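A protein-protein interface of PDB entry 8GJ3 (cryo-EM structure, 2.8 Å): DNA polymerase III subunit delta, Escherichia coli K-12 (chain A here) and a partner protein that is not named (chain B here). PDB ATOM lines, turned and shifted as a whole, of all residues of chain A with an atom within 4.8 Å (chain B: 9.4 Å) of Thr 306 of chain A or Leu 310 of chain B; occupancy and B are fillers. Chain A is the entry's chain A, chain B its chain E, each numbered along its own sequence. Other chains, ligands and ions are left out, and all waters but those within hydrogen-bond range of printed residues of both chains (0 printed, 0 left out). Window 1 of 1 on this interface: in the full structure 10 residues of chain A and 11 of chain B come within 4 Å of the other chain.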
ATOM      1  N   GLN A 251      -8.227  -1.880  17.601  1.00  0.00           N
ATOM      2  CA  GLN A 251      -8.197  -2.160  16.169  1.00  0.00           C
ATOM      3  C   GLN A 251      -7.231  -3.294  15.848  1.00  0.00           C
ATOM      4  O   GLN A 251      -7.571  -4.222  15.105  1.00  0.00           O
ATOM      5  CB  GLN A 251      -7.814  -0.894  15.399  1.00  0.00           C
ATOM      6  CG  GLN A 251      -7.762  -1.077  13.890  1.00  0.00           C
ATOM      7  CD  GLN A 251      -7.374   0.191  13.164  1.00  0.00           C
ATOM      8  OE1 GLN A 251      -7.328   1.271  13.753  1.00  0.00           O
ATOM      9  NE2 GLN A 251      -7.086   0.067  11.874  1.00  0.00           N
ATOM     10  N   LEU A 255      -8.720  -6.746  14.325  1.00  0.00           N
ATOM     11  CA  LEU A 255      -8.352  -7.151  12.972  1.00  0.00           C
ATOM     12  C   LEU A 255      -7.633  -8.493  12.978  1.00  0.00           C
ATOM     13  O   LEU A 255      -7.840  -9.322  12.085  1.00  0.00           O
ATOM     14  CB  LEU A 255      -7.479  -6.076  12.322  1.00  0.00           C
ATOM     15  CG  LEU A 255      -8.166  -4.736  12.046  1.00  0.00           C
ATOM     16  CD1 LEU A 255      -7.150  -3.701  11.591  1.00  0.00           C
ATOM     17  CD2 LEU A 255      -9.267  -4.893  11.011  1.00  0.00           C
ATOM     18  N   VAL A 302     -16.561  -4.617  13.494  1.00  0.00           N
ATOM     19  CA  VAL A 302     -15.768  -3.790  12.589  1.00  0.00           C
ATOM     20  C   VAL A 302     -16.612  -2.647  12.042  1.00  0.00           C
ATOM     21  O   VAL A 302     -16.158  -1.498  11.971  1.00  0.00           O
ATOM     22  CB  VAL A 302     -15.178  -4.649  11.456  1.00  0.00           C
ATOM     23  CG1 VAL A 302     -14.497  -3.769  10.420  1.00  0.00           C
ATOM     24  CG2 VAL A 302     -14.199  -5.667  12.016  1.00  0.00           C
ATOM     25  N   GLN A 303     -17.851  -2.942  11.642  1.00  0.00           N
ATOM     26  CA  GLN A 303     -18.722  -1.898  11.115  1.00  0.00           C
ATOM     27  C   GLN A 303     -19.015  -0.842  12.172  1.00  0.00           C
ATOM     28  O   GLN A 303     -18.985   0.360  11.885  1.00  0.00           O
ATOM     29  CB  GLN A 303     -20.020  -2.515  10.598  1.00  0.00           C
ATOM     30  CG  GLN A 303     -20.933  -1.531   9.889  1.00  0.00           C
ATOM     31  CD  GLN A 303     -22.138  -2.202   9.266  1.00  0.00           C
ATOM     32  OE1 GLN A 303     -22.447  -3.355   9.569  1.00  0.00           O
ATOM     33  NE2 GLN A 303     -22.826  -1.485   8.385  1.00  0.00           N
ATOM     34  N   LEU A 304     -19.301  -1.271  13.403  1.00  0.00           N
ATOM     35  CA  LEU A 304     -19.536  -0.314  14.478  1.00  0.00           C
ATOM     36  C   LEU A 304     -18.281   0.502  14.764  1.00  0.00           C
ATOM     37  O   LEU A 304     -18.355   1.717  14.978  1.00  0.00           O
ATOM     38  CB  LEU A 304     -20.000  -1.047  15.737  1.00  0.00           C
ATOM     39  CG  LEU A 304     -20.929  -0.282  16.685  1.00  0.00           C
ATOM     40  CD1 LEU A 304     -21.293  -1.152  17.876  1.00  0.00           C
ATOM     41  CD2 LEU A 304     -20.308   1.026  17.150  1.00  0.00           C
ATOM     42  N   LEU A 305     -17.118  -0.152  14.769  1.00  0.00           N
ATOM     43  CA  LEU A 305     -15.871   0.562  15.018  1.00  0.00           C
ATOM     44  C   LEU A 305     -15.605   1.597  13.931  1.00  0.00           C
ATOM     45  O   LEU A 305     -15.171   2.716  14.223  1.00  0.00           O
ATOM     46  CB  LEU A 305     -14.713  -0.433  15.109  1.00  0.00           C
ATOM     47  CG  LEU A 305     -13.321   0.143  15.382  1.00  0.00           C
ATOM     48  CD1 LEU A 305     -13.288   0.883  16.709  1.00  0.00           C
ATOM     49  CD2 LEU A 305     -12.279  -0.962  15.361  1.00  0.00           C
ATOM     50  N   THR A 306     -15.860   1.239  12.670  1.00  0.00           N
ATOM     51  CA  THR A 306     -15.609   2.170  11.575  1.00  0.00           C
ATOM     52  C   THR A 306     -16.491   3.407  11.688  1.00  0.00           C
ATOM     53  O   THR A 306     -16.020   4.533  11.487  1.00  0.00           O
ATOM     54  CB  THR A 306     -15.837   1.475  10.234  1.00  0.00           C
ATOM     55  OG1 THR A 306     -15.005   0.311  10.148  1.00  0.00           O
ATOM     56  CG2 THR A 306     -15.510   2.412   9.081  1.00  0.00           C
ATOM     57  N   ARG A 307     -17.774   3.221  12.006  1.00  0.00           N
ATOM     58  CA  ARG A 307     -18.671   4.365  12.131  1.00  0.00           C
ATOM     59  C   ARG A 307     -18.237   5.277  13.271  1.00  0.00           C
ATOM     60  O   ARG A 307     -18.290   6.506  13.147  1.00  0.00           O
ATOM     61  CB  ARG A 307     -20.109   3.892  12.342  1.00  0.00           C
ATOM     62  CG  ARG A 307     -21.141   4.992  12.145  1.00  0.00           C
ATOM     63  CD  ARG A 307     -22.569   4.480  12.277  1.00  0.00           C
ATOM     64  NE  ARG A 307     -22.994   4.363  13.668  1.00  0.00           N
ATOM     65  CZ  ARG A 307     -22.874   3.271  14.412  1.00  0.00           C
ATOM     66  NH1 ARG A 307     -22.332   2.161  13.937  1.00  0.00           N
ATOM     67  NH2 ARG A 307     -23.311   3.292  15.668  1.00  0.00           N
ATOM     68  N   THR A 308     -17.807   4.693  14.390  1.00  0.00           N
ATOM     69  CA  THR A 308     -17.342   5.501  15.513  1.00  0.00           C
ATOM     70  C   THR A 308     -16.136   6.343  15.118  1.00  0.00           C
ATOM     71  O   THR A 308     -16.046   7.522  15.480  1.00  0.00           O
ATOM     72  CB  THR A 308     -16.998   4.600  16.700  1.00  0.00           C
ATOM     73  OG1 THR A 308     -18.125   3.777  17.022  1.00  0.00           O
ATOM     74  CG2 THR A 308     -16.621   5.434  17.916  1.00  0.00           C
ATOM     75  N   GLU A 309     -15.195   5.752  14.378  1.00  0.00           N
ATOM     76  CA  GLU A 309     -14.016   6.499  13.950  1.00  0.00           C
ATOM     77  C   GLU A 309     -14.401   7.675  13.062  1.00  0.00           C
ATOM     78  O   GLU A 309     -13.888   8.785  13.235  1.00  0.00           O
ATOM     79  CB  GLU A 309     -13.047   5.568  13.223  1.00  0.00           C
ATOM     80  CG  GLU A 309     -11.828   6.266  12.639  1.00  0.00           C
ATOM     81  CD  GLU A 309     -10.797   5.291  12.105  1.00  0.00           C
ATOM     82  OE1 GLU A 309     -10.758   4.140  12.587  1.00  0.00           O
ATOM     83  OE2 GLU A 309     -10.026   5.675  11.201  1.00  0.00           O
ATOM     84  N   LEU A 310     -15.308   7.452  12.108  1.00  0.00           N
ATOM     85  CA  LEU A 310     -15.712   8.533  11.215  1.00  0.00           C
ATOM     86  C   LEU A 310     -16.366   9.671  11.987  1.00  0.00           C
ATOM     87  O   LEU A 310     -16.098  10.847  11.720  1.00  0.00           O
ATOM     88  CB  LEU A 310     -16.662   8.000  10.142  1.00  0.00           C
ATOM     89  CG  LEU A 310     -16.036   7.109   9.067  1.00  0.00           C
ATOM     90  CD1 LEU A 310     -17.118   6.460   8.221  1.00  0.00           C
ATOM     91  CD2 LEU A 310     -15.084   7.907   8.191  1.00  0.00           C
ATOM     92  N   TYR B 230     -12.129 -10.575   0.341  1.00  0.00           N
ATOM     93  CA  TYR B 230     -11.233 -10.131   1.402  1.00  0.00           C
ATOM     94  C   TYR B 230      -9.768 -10.269   1.014  1.00  0.00           C
ATOM     95  O   TYR B 230      -8.923  -9.552   1.559  1.00  0.00           O
ATOM     96  CB  TYR B 230     -11.514 -10.919   2.682  1.00  0.00           C
ATOM     97  CG  TYR B 230     -10.656 -10.512   3.858  1.00  0.00           C
ATOM     98  CD1 TYR B 230     -10.855  -9.297   4.499  1.00  0.00           C
ATOM     99  CD2 TYR B 230      -9.653 -11.345   4.332  1.00  0.00           C
ATOM    100  CE1 TYR B 230     -10.075  -8.921   5.574  1.00  0.00           C
ATOM    101  CE2 TYR B 230      -8.868 -10.978   5.408  1.00  0.00           C
ATOM    102  CZ  TYR B 230      -9.084  -9.764   6.024  1.00  0.00           C
ATOM    103  OH  TYR B 230      -8.305  -9.394   7.095  1.00  0.00           O
ATOM    104  N   LEU B 233      -7.341  -7.182  -0.025  1.00  0.00           N
ATOM    105  CA  LEU B 233      -6.808  -6.176   0.888  1.00  0.00           C
ATOM    106  C   LEU B 233      -5.321  -5.944   0.647  1.00  0.00           C
ATOM    107  O   LEU B 233      -4.846  -4.804   0.707  1.00  0.00           O
ATOM    108  CB  LEU B 233      -7.056  -6.602   2.335  1.00  0.00           C
ATOM    109  CG  LEU B 233      -6.473  -5.701   3.426  1.00  0.00           C
ATOM    110  CD1 LEU B 233      -6.987  -4.277   3.290  1.00  0.00           C
ATOM    111  CD2 LEU B 233      -6.800  -6.258   4.800  1.00  0.00           C
ATOM    112  N   ASN B 237      -4.289  -2.139  -0.009  1.00  0.00           N
ATOM    113  CA  ASN B 237      -3.767  -1.410   1.144  1.00  0.00           C
ATOM    114  C   ASN B 237      -2.414  -0.814   0.779  1.00  0.00           C
ATOM    115  O   ASN B 237      -1.389  -1.501   0.802  1.00  0.00           O
ATOM    116  CB  ASN B 237      -3.656  -2.336   2.349  1.00  0.00           C
ATOM    117  CG  ASN B 237      -3.195  -1.612   3.599  1.00  0.00           C
ATOM    118  OD1 ASN B 237      -3.254  -0.385   3.676  1.00  0.00           O
ATOM    119  ND2 ASN B 237      -2.734  -2.371   4.585  1.00  0.00           N
ATOM    120  N   ILE B 296     -16.325   5.677  -0.575  1.00  0.00           N
ATOM    121  CA  ILE B 296     -15.214   5.461   0.347  1.00  0.00           C
ATOM    122  C   ILE B 296     -13.966   6.184  -0.146  1.00  0.00           C
ATOM    123  O   ILE B 296     -13.170   6.690   0.653  1.00  0.00           O
ATOM    124  CB  ILE B 296     -14.963   3.953   0.536  1.00  0.00           C
ATOM    125  CG1 ILE B 296     -13.938   3.715   1.647  1.00  0.00           C
ATOM    126  CG2 ILE B 296     -14.481   3.319  -0.755  1.00  0.00           C
ATOM    127  CD1 ILE B 296     -13.709   2.252   1.949  1.00  0.00           C
ATOM    128  N   GLN B 299     -14.148   9.787   1.011  1.00  0.00           N
ATOM    129  CA  GLN B 299     -13.838   9.914   2.433  1.00  0.00           C
ATOM    130  C   GLN B 299     -12.341   9.804   2.679  1.00  0.00           C
ATOM    131  O   GLN B 299     -11.777  10.563   3.477  1.00  0.00           O
ATOM    132  CB  GLN B 299     -14.588   8.848   3.231  1.00  0.00           C
ATOM    133  CG  GLN B 299     -16.077   9.104   3.364  1.00  0.00           C
ATOM    134  CD  GLN B 299     -16.780   8.025   4.161  1.00  0.00           C
ATOM    135  OE1 GLN B 299     -16.270   6.915   4.311  1.00  0.00           O
ATOM    136  NE2 GLN B 299     -17.957   8.348   4.684  1.00  0.00           N
ATOM    137  N   LEU B 300     -11.678   8.864   2.003  1.00  0.00           N
ATOM    138  CA  LEU B 300     -10.247   8.672   2.211  1.00  0.00           C
ATOM    139  C   LEU B 300      -9.462   9.917   1.818  1.00  0.00           C
ATOM    140  O   LEU B 300      -8.535  10.326   2.527  1.00  0.00           O
ATOM    141  CB  LEU B 300      -9.769   7.459   1.416  1.00  0.00           C
ATOM    142  CG  LEU B 300      -8.442   6.834   1.841  1.00  0.00           C
ATOM    143  CD1 LEU B 300      -8.563   6.195   3.216  1.00  0.00           C
ATOM    144  CD2 LEU B 300      -7.987   5.811   0.815  1.00  0.00           C
ATOM    145  N   VAL B 303     -11.308  13.214   4.321  1.00  0.00           N
ATOM    146  CA  VAL B 303     -11.088  13.189   5.762  1.00  0.00           C
ATOM    147  C   VAL B 303      -9.594  13.120   6.041  1.00  0.00           C
ATOM    148  O   VAL B 303      -8.878  12.281   5.479  1.00  0.00           O
ATOM    149  CB  VAL B 303     -11.830  12.007   6.402  1.00  0.00           C
ATOM    150  CG1 VAL B 303     -11.705  12.059   7.919  1.00  0.00           C
ATOM    151  CG2 VAL B 303     -13.294  12.005   5.985  1.00  0.00           C
ATOM    152  N   ILE B 306      -7.674   9.977   8.611  1.00  0.00           N
ATOM    153  CA  ILE B 306      -8.519   8.791   8.664  1.00  0.00           C
ATOM    154  C   ILE B 306      -7.667   7.554   8.418  1.00  0.00           C
ATOM    155  O   ILE B 306      -6.847   7.517   7.491  1.00  0.00           O
ATOM    156  CB  ILE B 306      -9.660   8.901   7.642  1.00  0.00           C
ATOM    157  CG1 ILE B 306     -10.684   7.778   7.840  1.00  0.00           C
ATOM    158  CG2 ILE B 306      -9.119   8.859   6.218  1.00  0.00           C
ATOM    159  CD1 ILE B 306     -11.441   7.852   9.148  1.00  0.00           C
ATOM    160  N   ASN B 307      -7.852   6.536   9.253  1.00  0.00           N
ATOM    161  CA  ASN B 307      -7.110   5.294   9.090  1.00  0.00           C
ATOM    162  C   ASN B 307      -7.496   4.623   7.778  1.00  0.00           C
ATOM    163  O   ASN B 307      -8.652   4.677   7.350  1.00  0.00           O
ATOM    164  CB  ASN B 307      -7.381   4.358  10.267  1.00  0.00           C
ATOM    165  CG  ASN B 307      -6.414   3.192  10.317  1.00  0.00           C
ATOM    166  OD1 ASN B 307      -6.175   2.523   9.313  1.00  0.00           O
ATOM    167  ND2 ASN B 307      -5.845   2.948  11.492  1.00  0.00           N
ATOM    168  N   ARG B 308      -6.516   3.984   7.140  1.00  0.00           N
ATOM    169  CA  ARG B 308      -6.713   3.415   5.812  1.00  0.00           C
ATOM    170  C   ARG B 308      -7.107   1.943   5.865  1.00  0.00           C
ATOM    171  O   ARG B 308      -8.044   1.525   5.177  1.00  0.00           O
ATOM    172  CB  ARG B 308      -5.438   3.585   4.982  1.00  0.00           C
ATOM    173  CG  ARG B 308      -5.609   3.253   3.509  1.00  0.00           C
ATOM    174  CD  ARG B 308      -4.283   3.268   2.764  1.00  0.00           C
ATOM    175  NE  ARG B 308      -3.560   4.525   2.934  1.00  0.00           N
ATOM    176  CZ  ARG B 308      -2.630   4.749   3.854  1.00  0.00           C
ATOM    177  NH1 ARG B 308      -2.272   3.818   4.725  1.00  0.00           N
ATOM    178  NH2 ARG B 308      -2.042   5.941   3.901  1.00  0.00           N
ATOM    179  N   GLU B 309      -6.402   1.144   6.669  1.00  0.00           N
ATOM    180  CA  GLU B 309      -6.656  -0.293   6.684  1.00  0.00           C
ATOM    181  C   GLU B 309      -8.069  -0.601   7.162  1.00  0.00           C
ATOM    182  O   GLU B 309      -8.736  -1.488   6.617  1.00  0.00           O
ATOM    183  CB  GLU B 309      -5.628  -0.998   7.566  1.00  0.00           C
ATOM    184  CG  GLU B 309      -5.733  -2.515   7.542  1.00  0.00           C
ATOM    185  CD  GLU B 309      -4.655  -3.189   8.368  1.00  0.00           C
ATOM    186  OE1 GLU B 309      -3.859  -2.470   9.008  1.00  0.00           O
ATOM    187  OE2 GLU B 309      -4.604  -4.436   8.377  1.00  0.00           O
ATOM    188  N   LEU B 310      -8.541   0.111   8.188  1.00  0.00           N
ATOM    189  CA  LEU B 310      -9.868  -0.168   8.723  1.00  0.00           C
ATOM    190  C   LEU B 310     -10.951   0.090   7.683  1.00  0.00           C
ATOM    191  O   LEU B 310     -11.875  -0.716   7.526  1.00  0.00           O
ATOM    192  CB  LEU B 310     -10.115   0.676   9.973  1.00  0.00           C
ATOM    193  CG  LEU B 310     -11.389   0.358  10.760  1.00  0.00           C
ATOM    194  CD1 LEU B 310     -11.328  -1.041  11.356  1.00  0.00           C
ATOM    195  CD2 LEU B 310     -11.614   1.395  11.846  1.00  0.00           C
ATOM    196  N   LEU B 311     -10.855   1.208   6.960  1.00  0.00           N
ATOM    197  CA  LEU B 311     -11.867   1.527   5.958  1.00  0.00           C
ATOM    198  C   LEU B 311     -11.893   0.483   4.850  1.00  0.00           C
ATOM    199  O   LEU B 311     -12.963   0.023   4.437  1.00  0.00           O
ATOM    200  CB  LEU B 311     -11.609   2.917   5.376  1.00  0.00           C
ATOM    201  CG  LEU B 311     -11.993   4.125   6.231  1.00  0.00           C
ATOM    202  CD1 LEU B 311     -11.565   5.405   5.531  1.00  0.00           C
ATOM    203  CD2 LEU B 311     -13.489   4.147   6.518  1.00  0.00           C
ATOM    204  N   ILE B 312     -10.717   0.092   4.355  1.00  0.00           N
ATOM    205  CA  ILE B 312     -10.664  -0.879   3.268  1.00  0.00           C
ATOM    206  C   ILE B 312     -11.117  -2.249   3.756  1.00  0.00           C
ATOM    207  O   ILE B 312     -11.799  -2.985   3.033  1.00  0.00           O
ATOM    208  CB  ILE B 312      -9.249  -0.927   2.662  1.00  0.00           C
ATOM    209  CG1 ILE B 312      -8.866   0.448   2.105  1.00  0.00           C
ATOM    210  CG2 ILE B 312      -9.177  -1.991   1.568  1.00  0.00           C
ATOM    211  CD1 ILE B 312      -7.425   0.557   1.657  1.00  0.00           C
ATOM    212  N   THR B 313     -10.743  -2.617   4.983  1.00  0.00           N
ATOM    213  CA  THR B 313     -11.174  -3.901   5.527  1.00  0.00           C
ATOM    214  C   THR B 313     -12.691  -3.959   5.655  1.00  0.00           C
ATOM    215  O   THR B 313     -13.312  -4.977   5.327  1.00  0.00           O
ATOM    216  CB  THR B 313     -10.517  -4.145   6.885  1.00  0.00           C
ATOM    217  OG1 THR B 313      -9.092  -4.096   6.746  1.00  0.00           O
ATOM    218  CG2 THR B 313     -10.922  -5.502   7.440  1.00  0.00           C
ATOM    219  N   ASP B 314     -13.306  -2.874   6.131  1.00  0.00           N
ATOM    220  CA  ASP B 314     -14.761  -2.833   6.221  1.00  0.00           C
ATOM    221  C   ASP B 314     -15.395  -2.917   4.838  1.00  0.00           C
ATOM    222  O   ASP B 314     -16.427  -3.574   4.659  1.00  0.00           O
ATOM    223  CB  ASP B 314     -15.203  -1.557   6.936  1.00  0.00           C
ATOM    224  CG  ASP B 314     -16.692  -1.534   7.222  1.00  0.00           C
ATOM    225  OD1 ASP B 314     -17.361  -2.563   6.993  1.00  0.00           O
ATOM    226  OD2 ASP B 314     -17.195  -0.485   7.675  1.00  0.00           O
ATOM    227  N   LEU B 315     -14.791  -2.257   3.849  1.00  0.00           N
ATOM    228  CA  LEU B 315     -15.336  -2.277   2.496  1.00  0.00           C
ATOM    229  C   LEU B 315     -15.421  -3.701   1.960  1.00  0.00           C
ATOM    230  O   LEU B 315     -16.469  -4.128   1.462  1.00  0.00           O
ATOM    231  CB  LEU B 315     -14.475  -1.409   1.579  1.00  0.00           C
ATOM    232  CG  LEU B 315     -14.871  -1.354   0.102  1.00  0.00           C
ATOM    233  CD1 LEU B 315     -16.224  -0.688  -0.068  1.00  0.00           C
ATOM    234  CD2 LEU B 315     -13.809  -0.631  -0.708  1.00  0.00           C
ATOM    235  N   LEU B 316     -14.324  -4.454   2.054  1.00  0.00           N
ATOM    236  CA  LEU B 316     -14.312  -5.807   1.507  1.00  0.00           C
ATOM    237  C   LEU B 316     -15.303  -6.705   2.233  1.00  0.00           C
ATOM    238  O   LEU B 316     -16.004  -7.505   1.602  1.00  0.00           O
ATOM    239  CB  LEU B 316     -12.900  -6.388   1.583  1.00  0.00           C
ATOM    240  CG  LEU B 316     -11.823  -5.625   0.810  1.00  0.00           C
ATOM    241  CD1 LEU B 316     -10.459  -6.248   1.048  1.00  0.00           C
ATOM    242  CD2 LEU B 316     -12.141  -5.589  -0.677  1.00  0.00           C
ATOM    243  N   LEU B 317     -15.374  -6.595   3.561  1.00  0.00           N
ATOM    244  CA  LEU B 317     -16.354  -7.374   4.309  1.00  0.00           C
ATOM    245  C   LEU B 317     -17.774  -6.968   3.939  1.00  0.00           C
ATOM    246  O   LEU B 317     -18.656  -7.822   3.793  1.00  0.00           O
ATOM    247  CB  LEU B 317     -16.120  -7.207   5.810  1.00  0.00           C
ATOM    248  CG  LEU B 317     -14.777  -7.717   6.340  1.00  0.00           C
ATOM    249  CD1 LEU B 317     -14.608  -7.343   7.802  1.00  0.00           C
ATOM    250  CD2 LEU B 317     -14.657  -9.221   6.157  1.00  0.00           C
ATOM    251  N   ARG B 318     -18.014  -5.664   3.784  1.00  0.00           N
ATOM    252  CA  ARG B 318     -19.338  -5.200   3.381  1.00  0.00           C
ATOM    253  C   ARG B 318     -19.705  -5.727   2.001  1.00  0.00           C
ATOM    254  O   ARG B 318     -20.841  -6.164   1.777  1.00  0.00           O
ATOM    255  CB  ARG B 318     -19.380  -3.673   3.397  1.00  0.00           C
ATOM    256  CG  ARG B 318     -20.767  -3.082   3.212  1.00  0.00           C
ATOM    257  CD  ARG B 318     -20.688  -1.606   2.863  1.00  0.00           C
ATOM    258  NE  ARG B 318     -19.882  -0.858   3.819  1.00  0.00           N
ATOM    259  CZ  ARG B 318     -19.561   0.423   3.691  1.00  0.00           C
ATOM    260  NH1 ARG B 318     -19.961   1.136   2.649  1.00  0.00           N
ATOM    261  NH2 ARG B 318     -18.819   1.002   4.629  1.00  0.00           N
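Among the printed residues, pairs that only touch across the chains: Glu 309 of chain A with Leu 310 of chain B, Glu 309 of chain A with Ile 306 of chain B, Gln 251 of chain A with Leu 310 of chain B, Thr 306 of chain A with Leu 310 of chain B, Thr 306 of chain A with Leu 311 of chain B, Leu 310 of chain A with Ile 306 of chain B and Leu 255 of chain A with Thr 313 of chain B.
Printed residues of chain B within 4 Å of Gln 251 of chain A: Asn 307 (3.2 Å) and Leu 310 (3.6 Å).
No residue of chain B comes within 4 Å of Leu 305 of chain A.
Of chain B, only Leu 310, Leu 311 and Asp 314 come within 4 Å of Thr 306 of chain A.
Printed residues of chain B within 4 Å of Leu 310 of chain A: Ile 306.
Asn 237 of chain B touches none of the printed residues of chain A.
Of the printed residues of chain A, Asn 307 of chain B touches Gln 251 (3.2 Å) and Glu 309 (3.0 Å).
Leu 310 of chain B touches just these residues of chain A: Gln 251, Thr 306 and Glu 309.
Of the printed residues of chain A, Leu 311 of chain B touches Thr 306.
Printed residues of chain A within 4 Å of Asp 314 of chain B: Thr 306.
The nearest residue of chain B that does not touch Thr 306 of chain A is Arg 318 of chain B (5.7 Å).
The nearest residue of chain A that does not touch Leu 310 of chain B is Leu 305 of chain A (4.1 Å).
ND2 of Asn 307 of chain B sits close to NE2 of Gln 251 of chain A (3.2 Å).
The side-chain carboxylate (OD2) of Asp 314 of chain B is in hydrogen-bond range of the side-chain hydroxyl (OG1) of Thr 306 of chain A (3.4 Å).
The backbone NH (N) of Asn 307 of chain B is in hydrogen-bond range of the side-chain carboxylate (OE2) of Glu 309 of chain A (3.0 Å).
The backbone carbonyl oxygen (O) of Val 302 of chain A is in hydrogen-bond range of the side-chain hydroxyl (OG1) of Thr 306 of chain A, at 2.8 Å.
OD1 of Asn 307 of chain B lies within hydrogen-bond range of N of Glu 309 of chain B.
O of Glu 309 of chain B sits at hydrogen-bond distance from OG1 of Thr 313 of chain B (2.6 Å).
OD2 of Asp 314 of chain B lies within salt-bridge range of NH2 of Arg 318 of chain B (3.8 Å).
Of the 11 printed residues of chain A, 5 touch a printed residue of chain B.
Hydrophobic or aromatic side chains of chain A within 4 Å of the printed part of chain B: Leu 255 and Leu 310.
Printed residues of chain B that touch a printed residue of chain A: Ile 306, Asn 307, Leu 310, Leu 311, Thr 313 and Asp 314.
Along chain B the printed residues that touch a printed residue of chain A span positions 306 to 314.
Among the printed residues, no Asp or Glu carboxylate lies within 4 Å of a Lys or Arg side-chain nitrogen of the other chain.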
